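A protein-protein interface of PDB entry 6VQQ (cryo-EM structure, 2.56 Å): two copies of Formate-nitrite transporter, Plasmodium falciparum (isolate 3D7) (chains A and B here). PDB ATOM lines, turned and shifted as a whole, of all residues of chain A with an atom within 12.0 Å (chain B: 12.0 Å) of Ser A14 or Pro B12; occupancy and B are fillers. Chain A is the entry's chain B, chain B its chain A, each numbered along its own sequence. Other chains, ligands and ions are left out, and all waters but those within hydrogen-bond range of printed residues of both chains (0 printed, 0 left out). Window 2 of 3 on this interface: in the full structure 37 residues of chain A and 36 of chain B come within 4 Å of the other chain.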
ATOM      1  N   PRO A  12      37.965   2.657  10.195  1.00  0.00           N
ATOM      2  CA  PRO A  12      36.825   1.759   9.995  1.00  0.00           C
ATOM      3  C   PRO A  12      36.172   1.331  11.308  1.00  0.00           C
ATOM      4  O   PRO A  12      36.864   0.859  12.209  1.00  0.00           O
ATOM      5  CB  PRO A  12      37.451   0.560   9.281  1.00  0.00           C
ATOM      6  CG  PRO A  12      38.596   1.137   8.528  1.00  0.00           C
ATOM      7  CD  PRO A  12      39.113   2.288   9.349  1.00  0.00           C
ATOM      8  N   VAL A  13      34.856   1.498  11.407  1.00  0.00           N
ATOM      9  CA  VAL A  13      34.093   1.139  12.596  1.00  0.00           C
ATOM     10  C   VAL A  13      32.909   0.289  12.161  1.00  0.00           C
ATOM     11  O   VAL A  13      32.387   0.463  11.054  1.00  0.00           O
ATOM     12  CB  VAL A  13      33.619   2.384  13.368  1.00  0.00           C
ATOM     13  CG1 VAL A  13      32.819   1.977  14.599  1.00  0.00           C
ATOM     14  CG2 VAL A  13      34.809   3.250  13.760  1.00  0.00           C
ATOM     15  N   SER A  14      32.487  -0.626  13.031  1.00  0.00           N
ATOM     16  CA  SER A  14      31.388  -1.520  12.699  1.00  0.00           C
ATOM     17  C   SER A  14      30.048  -0.853  12.980  1.00  0.00           C
ATOM     18  O   SER A  14      29.924  -0.031  13.893  1.00  0.00           O
ATOM     19  CB  SER A  14      31.504  -2.818  13.496  1.00  0.00           C
ATOM     20  OG  SER A  14      31.323  -2.585  14.882  1.00  0.00           O
ATOM     21  N   ILE A  15      29.041  -1.207  12.185  1.00  0.00           N
ATOM     22  CA  ILE A  15      27.677  -0.725  12.369  1.00  0.00           C
ATOM     23  C   ILE A  15      26.712  -1.849  12.019  1.00  0.00           C
ATOM     24  O   ILE A  15      26.830  -2.470  10.958  1.00  0.00           O
ATOM     25  CB  ILE A  15      27.390   0.530  11.518  1.00  0.00           C
ATOM     26  CG1 ILE A  15      27.644   0.262  10.033  1.00  0.00           C
ATOM     27  CG2 ILE A  15      28.232   1.704  11.993  1.00  0.00           C
ATOM     28  CD1 ILE A  15      27.178   1.377   9.131  1.00  0.00           C
ATOM     29  N   LYS A  16      25.770  -2.121  12.923  1.00  0.00           N
ATOM     30  CA  LYS A  16      24.698  -3.080  12.691  1.00  0.00           C
ATOM     31  C   LYS A  16      23.373  -2.441  13.073  1.00  0.00           C
ATOM     32  O   LYS A  16      23.254  -1.827  14.138  1.00  0.00           O
ATOM     33  CB  LYS A  16      24.913  -4.373  13.489  1.00  0.00           C
ATOM     34  CG  LYS A  16      25.080  -4.182  14.989  1.00  0.00           C
ATOM     35  CD  LYS A  16      25.812  -5.363  15.609  1.00  0.00           C
ATOM     36  CE  LYS A  16      25.853  -5.271  17.125  1.00  0.00           C
ATOM     37  NZ  LYS A  16      24.672  -5.922  17.756  1.00  0.00           N
ATOM     38  N   SER A  17      22.375  -2.596  12.206  1.00  0.00           N
ATOM     39  CA  SER A  17      21.112  -1.880  12.342  1.00  0.00           C
ATOM     40  C   SER A  17      20.017  -2.700  13.008  1.00  0.00           C
ATOM     41  O   SER A  17      19.271  -2.164  13.834  1.00  0.00           O
ATOM     42  CB  SER A  17      20.617  -1.420  10.967  1.00  0.00           C
ATOM     43  OG  SER A  17      20.331  -2.528  10.131  1.00  0.00           O
ATOM     44  N   VAL A  18      19.897  -3.980  12.678  1.00  0.00           N
ATOM     45  CA  VAL A  18      18.781  -4.794  13.141  1.00  0.00           C
ATOM     46  C   VAL A  18      19.162  -5.470  14.451  1.00  0.00           C
ATOM     47  O   VAL A  18      20.136  -6.230  14.511  1.00  0.00           O
ATOM     48  CB  VAL A  18      18.373  -5.831  12.079  1.00  0.00           C
ATOM     49  CG1 VAL A  18      19.502  -6.828  11.816  1.00  0.00           C
ATOM     50  CG2 VAL A  18      17.093  -6.554  12.504  1.00  0.00           C
ATOM     51  N   CYS A  19      18.398  -5.181  15.503  1.00  0.00           N
ATOM     52  CA  CYS A  19      18.514  -5.865  16.792  1.00  0.00           C
ATOM     53  C   CYS A  19      17.224  -6.661  16.967  1.00  0.00           C
ATOM     54  O   CYS A  19      16.248  -6.176  17.546  1.00  0.00           O
ATOM     55  CB  CYS A  19      18.749  -4.876  17.933  1.00  0.00           C
ATOM     56  SG  CYS A  19      17.492  -3.586  18.104  1.00  0.00           S
ATOM     57  N   GLU A  23      14.198  -7.162  21.436  1.00  0.00           N
ATOM     58  CA  GLU A  23      13.902  -5.749  21.224  1.00  0.00           C
ATOM     59  C   GLU A  23      12.620  -5.561  20.425  1.00  0.00           C
ATOM     60  O   GLU A  23      11.762  -4.751  20.797  1.00  0.00           O
ATOM     61  CB  GLU A  23      15.078  -5.078  20.517  1.00  0.00           C
ATOM     62  CG  GLU A  23      16.393  -5.157  21.289  1.00  0.00           C
ATOM     63  CD  GLU A  23      17.262  -6.335  20.880  1.00  0.00           C
ATOM     64  OE1 GLU A  23      16.933  -7.014  19.885  1.00  0.00           O
ATOM     65  OE2 GLU A  23      18.281  -6.582  21.559  1.00  0.00           O
ATOM     66  N   ASP A 208      16.449   0.181   9.100  1.00  0.00           N
ATOM     67  CA  ASP A 208      17.322   0.555   7.955  1.00  0.00           C
ATOM     68  C   ASP A 208      16.454   0.587   6.706  1.00  0.00           C
ATOM     69  O   ASP A 208      15.443  -0.096   6.652  1.00  0.00           O
ATOM     70  CB  ASP A 208      18.475  -0.410   7.847  1.00  0.00           C
ATOM     71  CG  ASP A 208      19.688   0.142   7.122  1.00  0.00           C
ATOM     72  OD1 ASP A 208      19.676   1.341   6.780  1.00  0.00           O
ATOM     73  OD2 ASP A 208      20.647  -0.624   6.893  1.00  0.00           O
ATOM     74  N   PRO B  12      30.291  -3.486  18.012  1.00  0.00           N
ATOM     75  CA  PRO B  12      28.830  -3.353  18.004  1.00  0.00           C
ATOM     76  C   PRO B  12      28.369  -1.902  18.097  1.00  0.00           C
ATOM     77  O   PRO B  12      28.916  -1.135  18.889  1.00  0.00           O
ATOM     78  CB  PRO B  12      28.404  -4.139  19.245  1.00  0.00           C
ATOM     79  CG  PRO B  12      29.569  -4.046  20.162  1.00  0.00           C
ATOM     80  CD  PRO B  12      30.787  -4.037  19.285  1.00  0.00           C
ATOM     81  N   VAL B  13      27.377  -1.533  17.290  1.00  0.00           N
ATOM     82  CA  VAL B  13      26.827  -0.184  17.278  1.00  0.00           C
ATOM     83  C   VAL B  13      25.342  -0.267  16.956  1.00  0.00           C
ATOM     84  O   VAL B  13      24.904  -1.161  16.225  1.00  0.00           O
ATOM     85  CB  VAL B  13      27.551   0.722  16.260  1.00  0.00           C
ATOM     86  CG1 VAL B  13      26.946   2.119  16.268  1.00  0.00           C
ATOM     87  CG2 VAL B  13      29.039   0.785  16.563  1.00  0.00           C
ATOM     88  N   SER B  14      24.571   0.667  17.506  1.00  0.00           N
ATOM     89  CA  SER B  14      23.138   0.743  17.260  1.00  0.00           C
ATOM     90  C   SER B  14      22.873   1.814  16.210  1.00  0.00           C
ATOM     91  O   SER B  14      23.439   2.911  16.281  1.00  0.00           O
ATOM     92  CB  SER B  14      22.385   1.055  18.550  1.00  0.00           C
ATOM     93  OG  SER B  14      22.773   0.176  19.591  1.00  0.00           O
ATOM     94  N   ILE B  15      22.021   1.498  15.239  1.00  0.00           N
ATOM     95  CA  ILE B  15      21.753   2.378  14.110  1.00  0.00           C
ATOM     96  C   ILE B  15      20.254   2.444  13.866  1.00  0.00           C
ATOM     97  O   ILE B  15      19.557   1.425  13.926  1.00  0.00           O
ATOM     98  CB  ILE B  15      22.488   1.901  12.839  1.00  0.00           C
ATOM     99  CG1 ILE B  15      24.000   2.016  13.031  1.00  0.00           C
ATOM    100  CG2 ILE B  15      22.030   2.698  11.626  1.00  0.00           C
ATOM    101  CD1 ILE B  15      24.638   0.756  13.546  1.00  0.00           C
ATOM    102  N   LYS B  16      19.760   3.651  13.593  1.00  0.00           N
ATOM    103  CA  LYS B  16      18.383   3.874  13.159  1.00  0.00           C
ATOM    104  C   LYS B  16      18.430   4.920  12.053  1.00  0.00           C
ATOM    105  O   LYS B  16      18.325   6.120  12.322  1.00  0.00           O
ATOM    106  CB  LYS B  16      17.495   4.329  14.311  1.00  0.00           C
ATOM    107  CG  LYS B  16      16.046   4.594  13.916  1.00  0.00           C
ATOM    108  CD  LYS B  16      15.335   5.486  14.925  1.00  0.00           C
ATOM    109  CE  LYS B  16      15.875   6.907  14.898  1.00  0.00           C
ATOM    110  NZ  LYS B  16      14.951   7.866  15.554  1.00  0.00           N
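N of Pro B12 sits close to OG of Ser A14, at 3.4 Å.
The backbone carbonyl oxygen of Val B13 lies close to the backbone carbonyl oxygen of Lys A16 (2.7 Å).
Of the 5 printed residues of chain B, 3 touch a printed residue of chain A.
Among the printed residues, no Asp or Glu carboxylate lies within 4 Å of a Lys or Arg side-chain nitrogen of the other chain.
Ser A14 touches Pro B12, but with the chains exchanged Pro A12 does not touch Ser B14 (13.2 Å).
Ile B15 touches its own counterpart, Ile A15.
Lys A16 touches Pro B12, but with the chains exchanged Pro A12 does not touch Lys B16 (16.7 Å).
Lys A16 touches Val B13, but with the chains exchanged Val A13 does not touch Lys B16 (13.2 Å).
5 positions are printed for both chains.
Of the 7 pairs that touch across the chains among the printed residues, 1 has its exchanged pair printed and touching as well.
Among the printed residues, merely in contact across the chains: Ser A14 with Val B13, Ile A15 with Ile B15, Lys A16 with Pro B12, Lys A16 with Ile B15 and Ser A17 with Ile B15.
Pro A12 touches none of the printed residues of chain B.
No residue of chain B comes within 4 Å of Val A13.
Lys A16 touches just these residues of chain B: Pro B12, Val B13 and Ile B15.
Printed residues of chain B within 4 Å of Ser A17: Ile B15.
Asp A208 touches none of the printed residues of chain B.
Val B13 touches just these residues of chain A: Ser A14 (2.9 Å) and Lys A16 (2.7 Å).
Of the printed residues of chain A, Ile B15 touches Ile A15, Lys A16 and Ser A17.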
